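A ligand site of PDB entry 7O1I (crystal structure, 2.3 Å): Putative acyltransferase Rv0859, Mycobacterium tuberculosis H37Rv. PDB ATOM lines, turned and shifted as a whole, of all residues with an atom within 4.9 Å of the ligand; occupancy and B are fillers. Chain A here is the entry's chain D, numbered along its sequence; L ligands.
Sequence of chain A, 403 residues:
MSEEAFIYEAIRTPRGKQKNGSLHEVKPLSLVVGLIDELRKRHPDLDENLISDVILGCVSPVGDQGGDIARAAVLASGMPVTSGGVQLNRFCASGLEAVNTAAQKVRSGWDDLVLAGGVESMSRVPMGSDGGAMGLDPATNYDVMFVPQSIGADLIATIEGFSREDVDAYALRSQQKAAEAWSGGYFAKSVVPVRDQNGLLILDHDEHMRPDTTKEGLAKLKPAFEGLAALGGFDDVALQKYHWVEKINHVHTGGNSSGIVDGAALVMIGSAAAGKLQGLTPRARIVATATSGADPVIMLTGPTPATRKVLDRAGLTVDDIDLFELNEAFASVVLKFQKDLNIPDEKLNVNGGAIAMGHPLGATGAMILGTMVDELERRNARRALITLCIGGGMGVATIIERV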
ATOM      1  N   GLN A  18     -13.003  32.692   3.416  1.00  0.00           N
ATOM      2  CA  GLN A  18     -12.245  33.917   3.661  1.00  0.00           C
ATOM      3  C   GLN A  18     -10.968  33.957   2.829  1.00  0.00           C
ATOM      4  O   GLN A  18     -10.751  34.896   2.053  1.00  0.00           O
ATOM      5  CB  GLN A  18     -11.918  34.027   5.150  1.00  0.00           C
ATOM      6  CG  GLN A  18     -11.131  35.271   5.533  1.00  0.00           C
ATOM      7  CD  GLN A  18     -10.682  35.249   6.978  1.00  0.00           C
ATOM      8  OE1 GLN A  18     -10.821  36.232   7.693  1.00  0.00           O
ATOM      9  NE2 GLN A  18     -10.123  34.121   7.407  1.00  0.00           N
ATOM     10  N   CSO A  92     -24.629  38.922  15.413  1.00  0.00           N
ATOM     11  CA  CSO A  92     -24.885  37.779  14.528  1.00  0.00           C
ATOM     12  CB  CSO A  92     -23.935  36.620  14.870  1.00  0.00           C
ATOM     13  SG  CSO A  92     -23.064  36.933  16.425  1.00  0.00           S
ATOM     14  C   CSO A  92     -26.341  37.295  14.518  1.00  0.00           C
ATOM     15  O   CSO A  92     -26.643  36.290  13.887  1.00  0.00           O
ATOM     16  OD  CSO A  92     -22.078  35.526  16.908  1.00  0.00           O
ATOM     17  N   MET A 127     -14.117  41.507  10.727  1.00  0.00           N
ATOM     18  CA  MET A 127     -14.810  41.635  12.012  1.00  0.00           C
ATOM     19  C   MET A 127     -14.264  42.814  12.809  1.00  0.00           C
ATOM     20  O   MET A 127     -13.050  43.062  12.824  1.00  0.00           O
ATOM     21  CB  MET A 127     -14.671  40.358  12.833  1.00  0.00           C
ATOM     22  CG  MET A 127     -15.485  39.187  12.334  1.00  0.00           C
ATOM     23  SD  MET A 127     -15.144  37.684  13.268  1.00  0.00           S
ATOM     24  CE  MET A 127     -15.252  38.303  14.943  1.00  0.00           C
ATOM     25  N   GLN A 149     -15.952  36.166  22.254  1.00  0.00           N
ATOM     26  CA  GLN A 149     -16.920  35.081  22.230  1.00  0.00           C
ATOM     27  C   GLN A 149     -16.254  33.714  22.290  1.00  0.00           C
ATOM     28  O   GLN A 149     -16.832  32.763  22.822  1.00  0.00           O
ATOM     29  CB  GLN A 149     -17.809  35.188  20.981  1.00  0.00           C
ATOM     30  CG  GLN A 149     -17.077  35.001  19.648  1.00  0.00           C
ATOM     31  CD  GLN A 149     -16.198  36.172  19.263  1.00  0.00           C
ATOM     32  OE1 GLN A 149     -16.270  37.240  19.877  1.00  0.00           O
ATOM     33  NE2 GLN A 149     -15.371  35.978  18.248  1.00  0.00           N
ATOM     34  N   GLN A 175     -20.162  18.600   9.433  1.00  0.00           N
ATOM     35  CA  GLN A 175     -19.628  18.405   8.091  1.00  0.00           C
ATOM     36  C   GLN A 175     -20.392  17.335   7.344  1.00  0.00           C
ATOM     37  O   GLN A 175     -20.663  17.468   6.144  1.00  0.00           O
ATOM     38  CB  GLN A 175     -18.143  18.046   8.169  1.00  0.00           C
ATOM     39  CG  GLN A 175     -17.254  19.115   8.774  1.00  0.00           C
ATOM     40  CD  GLN A 175     -16.984  20.265   7.822  1.00  0.00           C
ATOM     41  OE1 GLN A 175     -17.474  20.278   6.687  1.00  0.00           O
ATOM     42  NE2 GLN A 175     -16.201  21.236   8.270  1.00  0.00           N
ATOM     43  N   ARG A 210     -15.638  21.075   4.257  1.00  0.00           N
ATOM     44  CA  ARG A 210     -14.605  20.060   4.112  1.00  0.00           C
ATOM     45  C   ARG A 210     -15.279  18.704   4.306  1.00  0.00           C
ATOM     46  O   ARG A 210     -15.271  18.150   5.408  1.00  0.00           O
ATOM     47  CB  ARG A 210     -13.461  20.260   5.101  1.00  0.00           C
ATOM     48  CG  ARG A 210     -12.740  21.593   4.969  1.00  0.00           C
ATOM     49  CD  ARG A 210     -11.863  21.835   6.187  1.00  0.00           C
ATOM     50  NE  ARG A 210     -11.059  23.054   6.059  1.00  0.00           N
ATOM     51  CZ  ARG A 210      -9.782  23.064   5.693  1.00  0.00           C
ATOM     52  NH1 ARG A 210      -9.156  21.926   5.420  1.00  0.00           N
ATOM     53  NH2 ARG A 210      -9.131  24.211   5.609  1.00  0.00           N
ATOM     54  N   THR A 213     -13.555  15.401   6.134  1.00  0.00           N
ATOM     55  CA  THR A 213     -12.943  15.552   7.444  1.00  0.00           C
ATOM     56  C   THR A 213     -13.097  14.274   8.263  1.00  0.00           C
ATOM     57  O   THR A 213     -14.167  13.656   8.286  1.00  0.00           O
ATOM     58  CB  THR A 213     -13.569  16.720   8.214  1.00  0.00           C
ATOM     59  OG1 THR A 213     -14.994  16.708   8.047  1.00  0.00           O
ATOM     60  CG2 THR A 213     -13.005  18.027   7.713  1.00  0.00           C
ATOM     61  N   GLY A 217      -8.470  13.754  12.060  1.00  0.00           N
ATOM     62  CA  GLY A 217      -7.958  14.999  11.525  1.00  0.00           C
ATOM     63  C   GLY A 217      -8.332  16.205  12.365  1.00  0.00           C
ATOM     64  O   GLY A 217      -7.574  17.184  12.412  1.00  0.00           O
ATOM     65  N   LEU A 218      -9.490  16.164  13.025  1.00  0.00           N
ATOM     66  CA  LEU A 218      -9.881  17.260  13.906  1.00  0.00           C
ATOM     67  C   LEU A 218      -9.041  17.274  15.175  1.00  0.00           C
ATOM     68  O   LEU A 218      -8.710  18.344  15.702  1.00  0.00           O
ATOM     69  CB  LEU A 218     -11.368  17.159  14.244  1.00  0.00           C
ATOM     70  CG  LEU A 218     -12.351  17.329  13.095  1.00  0.00           C
ATOM     71  CD1 LEU A 218     -13.734  16.877  13.519  1.00  0.00           C
ATOM     72  CD2 LEU A 218     -12.373  18.779  12.624  1.00  0.00           C
ATOM     73  N   LEU A 221      -5.790  19.348  15.194  1.00  0.00           N
ATOM     74  CA  LEU A 221      -5.824  20.797  15.161  1.00  0.00           C
ATOM     75  C   LEU A 221      -5.471  21.376  16.524  1.00  0.00           C
ATOM     76  O   LEU A 221      -5.659  20.736  17.566  1.00  0.00           O
ATOM     77  CB  LEU A 221      -7.213  21.286  14.725  1.00  0.00           C
ATOM     78  CG  LEU A 221      -7.723  20.728  13.399  1.00  0.00           C
ATOM     79  CD1 LEU A 221      -9.003  21.450  12.970  1.00  0.00           C
ATOM     80  CD2 LEU A 221      -6.657  20.824  12.319  1.00  0.00           C
ATOM     81  N   ALA A 224      -7.163  27.463  18.557  1.00  0.00           N
ATOM     82  CA  ALA A 224      -6.786  28.704  17.893  1.00  0.00           C
ATOM     83  C   ALA A 224      -6.843  29.910  18.822  1.00  0.00           C
ATOM     84  O   ALA A 224      -6.267  30.952  18.485  1.00  0.00           O
ATOM     85  CB  ALA A 224      -7.701  28.937  16.682  1.00  0.00           C
ATOM     86  N   PHE A 225      -7.507  29.797  19.965  1.00  0.00           N
ATOM     87  CA  PHE A 225      -7.694  30.931  20.874  1.00  0.00           C
ATOM     88  C   PHE A 225      -6.840  30.804  22.137  1.00  0.00           C
ATOM     89  O   PHE A 225      -7.173  31.399  23.160  1.00  0.00           O
ATOM     90  CB  PHE A 225      -9.168  31.069  21.225  1.00  0.00           C
ATOM     91  CG  PHE A 225     -10.092  30.957  20.049  1.00  0.00           C
ATOM     92  CD1 PHE A 225     -10.164  31.980  19.110  1.00  0.00           C
ATOM     93  CD2 PHE A 225     -10.878  29.835  19.862  1.00  0.00           C
ATOM     94  CE1 PHE A 225     -11.006  31.882  18.012  1.00  0.00           C
ATOM     95  CE2 PHE A 225     -11.729  29.734  18.775  1.00  0.00           C
ATOM     96  CZ  PHE A 225     -11.789  30.760  17.845  1.00  0.00           C
ATOM     97  N   THR A 253     -11.280  25.030  18.047  1.00  0.00           N
ATOM     98  CA  THR A 253     -10.237  25.219  17.044  1.00  0.00           C
ATOM     99  C   THR A 253     -10.847  25.658  15.716  1.00  0.00           C
ATOM    100  O   THR A 253     -12.020  26.032  15.658  1.00  0.00           O
ATOM    101  CB  THR A 253      -9.434  23.934  16.851  1.00  0.00           C
ATOM    102  OG1 THR A 253      -8.463  24.147  15.830  1.00  0.00           O
ATOM    103  CG2 THR A 253     -10.369  22.799  16.434  1.00  0.00           C
ATOM    104  N   GLY A 254     -10.068  25.611  14.642  1.00  0.00           N
ATOM    105  CA  GLY A 254     -10.608  25.952  13.340  1.00  0.00           C
ATOM    106  C   GLY A 254     -11.639  24.966  12.822  1.00  0.00           C
ATOM    107  O   GLY A 254     -12.485  25.335  11.998  1.00  0.00           O
ATOM    108  N   GLY A 255     -11.596  23.728  13.304  1.00  0.00           N
ATOM    109  CA  GLY A 255     -12.474  22.685  12.809  1.00  0.00           C
ATOM    110  C   GLY A 255     -13.824  22.627  13.480  1.00  0.00           C
ATOM    111  O   GLY A 255     -14.791  22.179  12.862  1.00  0.00           O
ATOM    112  N   SER A 257     -15.252  25.461  15.122  1.00  0.00           N
ATOM    113  CA  SER A 257     -15.804  26.805  15.214  1.00  0.00           C
ATOM    114  C   SER A 257     -16.353  27.230  13.855  1.00  0.00           C
ATOM    115  O   SER A 257     -15.974  26.689  12.816  1.00  0.00           O
ATOM    116  CB  SER A 257     -14.763  27.816  15.701  1.00  0.00           C
ATOM    117  OG  SER A 257     -14.244  27.451  16.965  1.00  0.00           O
ATOM    118  N   SER A 258     -17.242  28.217  13.874  1.00  0.00           N
ATOM    119  CA  SER A 258     -17.838  28.695  12.636  1.00  0.00           C
ATOM    120  C   SER A 258     -16.787  29.323  11.734  1.00  0.00           C
ATOM    121  O   SER A 258     -15.809  29.917  12.202  1.00  0.00           O
ATOM    122  CB  SER A 258     -18.949  29.701  12.936  1.00  0.00           C
ATOM    123  OG  SER A 258     -18.432  30.874  13.545  1.00  0.00           O
ATOM    124  N   GLY A 259     -16.982  29.173  10.424  1.00  0.00           N
ATOM    125  CA  GLY A 259     -16.052  29.703   9.458  1.00  0.00           C
ATOM    126  C   GLY A 259     -16.354  31.146   9.116  1.00  0.00           C
ATOM    127  O   GLY A 259     -17.502  31.593   9.135  1.00  0.00           O
ATOM    128  N   ILE A 260     -15.291  31.885   8.792  1.00  0.00           N
ATOM    129  CA  ILE A 260     -15.398  33.261   8.323  1.00  0.00           C
ATOM    130  C   ILE A 260     -15.642  33.224   6.822  1.00  0.00           C
ATOM    131  O   ILE A 260     -14.731  32.891   6.043  1.00  0.00           O
ATOM    132  CB  ILE A 260     -14.129  34.060   8.655  1.00  0.00           C
ATOM    133  CG1 ILE A 260     -13.971  34.198  10.174  1.00  0.00           C
ATOM    134  CG2 ILE A 260     -14.153  35.429   7.980  1.00  0.00           C
ATOM    135  CD1 ILE A 260     -12.664  34.826  10.597  1.00  0.00           C
ATOM    136  N   ALA A 329     -21.947  28.850  15.915  1.00  0.00           N
ATOM    137  CA  ALA A 329     -20.831  29.763  16.133  1.00  0.00           C
ATOM    138  C   ALA A 329     -19.668  29.029  16.784  1.00  0.00           C
ATOM    139  O   ALA A 329     -18.507  29.178  16.380  1.00  0.00           O
ATOM    140  CB  ALA A 329     -21.271  30.952  16.984  1.00  0.00           C
ATOM    141  N   PHE A 330     -19.964  28.220  17.799  1.00  0.00           N
ATOM    142  CA  PHE A 330     -19.004  27.314  18.409  1.00  0.00           C
ATOM    143  C   PHE A 330     -19.742  26.034  18.778  1.00  0.00           C
ATOM    144  O   PHE A 330     -20.944  26.048  19.061  1.00  0.00           O
ATOM    145  CB  PHE A 330     -18.341  27.915  19.650  1.00  0.00           C
ATOM    146  CG  PHE A 330     -17.523  29.138  19.358  1.00  0.00           C
ATOM    147  CD1 PHE A 330     -16.199  29.018  18.951  1.00  0.00           C
ATOM    148  CD2 PHE A 330     -18.068  30.399  19.488  1.00  0.00           C
ATOM    149  CE1 PHE A 330     -15.446  30.141  18.677  1.00  0.00           C
ATOM    150  CE2 PHE A 330     -17.317  31.531  19.215  1.00  0.00           C
ATOM    151  CZ  PHE A 330     -16.000  31.399  18.808  1.00  0.00           C
ATOM    152  N   HIS A 359     -20.295  31.232   8.480  1.00  0.00           N
ATOM    153  CA  HIS A 359     -21.111  32.122   9.316  1.00  0.00           C
ATOM    154  C   HIS A 359     -20.960  33.561   8.867  1.00  0.00           C
ATOM    155  O   HIS A 359     -20.150  34.326   9.407  1.00  0.00           O
ATOM    156  CB  HIS A 359     -20.728  31.968  10.790  1.00  0.00           C
ATOM    157  CG  HIS A 359     -21.448  32.907  11.713  1.00  0.00           C
ATOM    158  ND1 HIS A 359     -22.826  32.975  11.773  1.00  0.00           N
ATOM    159  CD2 HIS A 359     -20.985  33.812  12.599  1.00  0.00           C
ATOM    160  CE1 HIS A 359     -23.178  33.883  12.664  1.00  0.00           C
ATOM    161  NE2 HIS A 359     -22.078  34.402  13.181  1.00  0.00           N
ATOM    162  N   LEU A 361     -22.029  36.986   9.275  1.00  0.00           N
ATOM    163  CA  LEU A 361     -22.675  37.492  10.480  1.00  0.00           C
ATOM    164  C   LEU A 361     -24.052  38.076  10.206  1.00  0.00           C
ATOM    165  O   LEU A 361     -25.074  37.555  10.681  1.00  0.00           O
ATOM    166  CB  LEU A 361     -21.774  38.541  11.133  1.00  0.00           C
ATOM    167  CG  LEU A 361     -20.291  38.206  11.303  1.00  0.00           C
ATOM    168  CD1 LEU A 361     -19.505  39.437  11.726  1.00  0.00           C
ATOM    169  CD2 LEU A 361     -20.101  37.085  12.301  1.00  0.00           C
HETATM  170  N1  LIG L   1     -10.533  19.601   9.159  1.00  0.00           N
HETATM  171  C1  LIG L   1      -9.199  19.689   9.079  1.00  0.00           C
HETATM  172  N2  LIG L   1      -8.419  20.761   9.216  1.00  0.00           N
HETATM  173  C2  LIG L   1      -9.152  21.854   9.465  1.00  0.00           C
HETATM  174  C3  LIG L   1     -10.529  21.918   9.585  1.00  0.00           C
HETATM  175  C4  LIG L   1     -11.239  20.720   9.424  1.00  0.00           C
HETATM  176  N3  LIG L   1     -12.575  20.641   9.504  1.00  0.00           N
HETATM  177  N4  LIG L   1     -10.928  23.226   9.854  1.00  0.00           N
HETATM  178  C5  LIG L   1      -9.811  23.913   9.905  1.00  0.00           C
HETATM  179  N5  LIG L   1      -8.704  23.128   9.682  1.00  0.00           N
HETATM  180  C6  LIG L   1      -7.311  23.579   9.641  1.00  0.00           C
HETATM  181  C7  LIG L   1      -6.965  24.374   8.394  1.00  0.00           C
HETATM  182  O1  LIG L   1      -6.698  23.563   7.266  1.00  0.00           O
HETATM  183  C8  LIG L   1      -5.775  25.206   8.872  1.00  0.00           C
HETATM  184  O2  LIG L   1      -4.572  24.461   8.725  1.00  0.00           O
HETATM  185  P1  LIG L   1      -3.553  25.348   7.843  1.00  0.00           P
HETATM  186  O3  LIG L   1      -2.270  24.540   7.701  1.00  0.00           O
HETATM  187  O4  LIG L   1      -4.227  25.586   6.511  1.00  0.00           O
HETATM  188  O5  LIG L   1      -3.323  26.636   8.605  1.00  0.00           O
HETATM  189  C9  LIG L   1      -6.083  25.427  10.359  1.00  0.00           C
HETATM  190  O6  LIG L   1      -7.116  24.467  10.713  1.00  0.00           O
HETATM  191  C10 LIG L   1      -6.580  26.809  10.716  1.00  0.00           C
HETATM  192  O7  LIG L   1      -7.956  26.938  10.301  1.00  0.00           O
HETATM  193  P2  LIG L   1      -8.326  27.857   9.034  1.00  0.00           P
HETATM  194  O8  LIG L   1      -9.411  27.194   8.248  1.00  0.00           O
HETATM  195  O9  LIG L   1      -7.069  28.255   8.326  1.00  0.00           O
HETATM  196  O10 LIG L   1      -8.958  29.140   9.757  1.00  0.00           O
HETATM  197  P3  LIG L   1      -8.375  30.285  10.730  1.00  0.00           P
HETATM  198  O11 LIG L   1      -6.965  29.951  11.095  1.00  0.00           O
HETATM  199  O12 LIG L   1      -8.668  31.623  10.150  1.00  0.00           O
HETATM  200  O13 LIG L   1      -9.285  30.100  12.045  1.00  0.00           O
HETATM  201  C11 LIG L   1     -11.320  30.100  13.360  1.00  0.00           C
HETATM  202  C12 LIG L   1     -10.717  30.379  11.977  1.00  0.00           C
HETATM  203  C13 LIG L   1     -12.532  29.180  13.187  1.00  0.00           C
HETATM  204  C14 LIG L   1     -10.283  29.373  14.214  1.00  0.00           C
HETATM  205  C15 LIG L   1     -11.746  31.383  14.068  1.00  0.00           C
HETATM  206  O14 LIG L   1     -10.754  32.392  13.925  1.00  0.00           O
HETATM  207  C16 LIG L   1     -13.109  31.918  13.670  1.00  0.00           C
HETATM  208  O15 LIG L   1     -13.374  32.123  12.492  1.00  0.00           O
HETATM  209  N6  LIG L   1     -13.969  32.178  14.651  1.00  0.00           N
HETATM  210  C17 LIG L   1     -15.340  32.616  14.435  1.00  0.00           C
HETATM  211  C18 LIG L   1     -15.558  34.065  14.818  1.00  0.00           C
HETATM  212  C19 LIG L   1     -16.998  34.357  15.168  1.00  0.00           C
HETATM  213  O16 LIG L   1     -17.793  33.434  15.372  1.00  0.00           O
HETATM  214  N7  LIG L   1     -17.381  35.641  15.240  1.00  0.00           N
HETATM  215  C20 LIG L   1     -18.684  36.051  15.722  1.00  0.00           C
HETATM  216  C21 LIG L   1     -18.617  37.158  16.739  1.00  0.00           C
HETATM  217  S1  LIG L   1     -18.651  38.808  16.001  1.00  0.00           S
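The side-chain hydroxyl of Ser 258 is in hydrogen-bond range of an oxygen (O16) of the ligand (3.2 Å). The side-chain sulfur (SD) of Met 127 lies close to a nitrogen (N7) of the ligand. The guanidinium group of Arg 210 lies within salt-bridge range of an oxygen (O8) of the ligand, at 3.99 Å.
The backbone carbonyl oxygen (O) of Arg 210 lies within hydrogen-bond range of the side-chain hydroxyl (OG1) of Thr 213 (3.0 Å). O of Ala 329 sits at hydrogen-bond distance from N of Ser 258, 3.0 Å away. The side-chain amide oxygen (OE1) of Gln 175 lies within hydrogen-bond range of the backbone NH (N) of Arg 210, at 3.1 Å. The backbone carbonyl oxygen (O) of Thr 253 lies within hydrogen-bond range of the side-chain hydroxyl (OG) of Ser 257 (2.9 Å). The backbone carbonyl oxygen (O) of Ile 260 is in hydrogen-bond range of the backbone NH (N) of Gln 18, at 3.2 Å.
N4 of the ligand sits close to O of Gly 254, at 3.4 Å. Residues that only touch the ligand: Ile 260 (3.2 Å), Thr 213 (3.2 Å), Gly 255 (3.4 Å), Leu 221 (3.5 Å), Ala 224 (3.6 Å), Ser 257 (3.6 Å), Gln 149 (3.6 Å), CSO 92 (3.6 Å), Leu 218 (3.6 Å), Phe 225 (3.8 Å), Leu 361 (3.8 Å), Gln 175 (3.9 Å) and Gln 18 (3.99 Å). Of the 23 residues printed, 17 come within 4 Å of the ligand. The nearest printed residue that does not touch the ligand is Thr 253 (4.03 Å).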
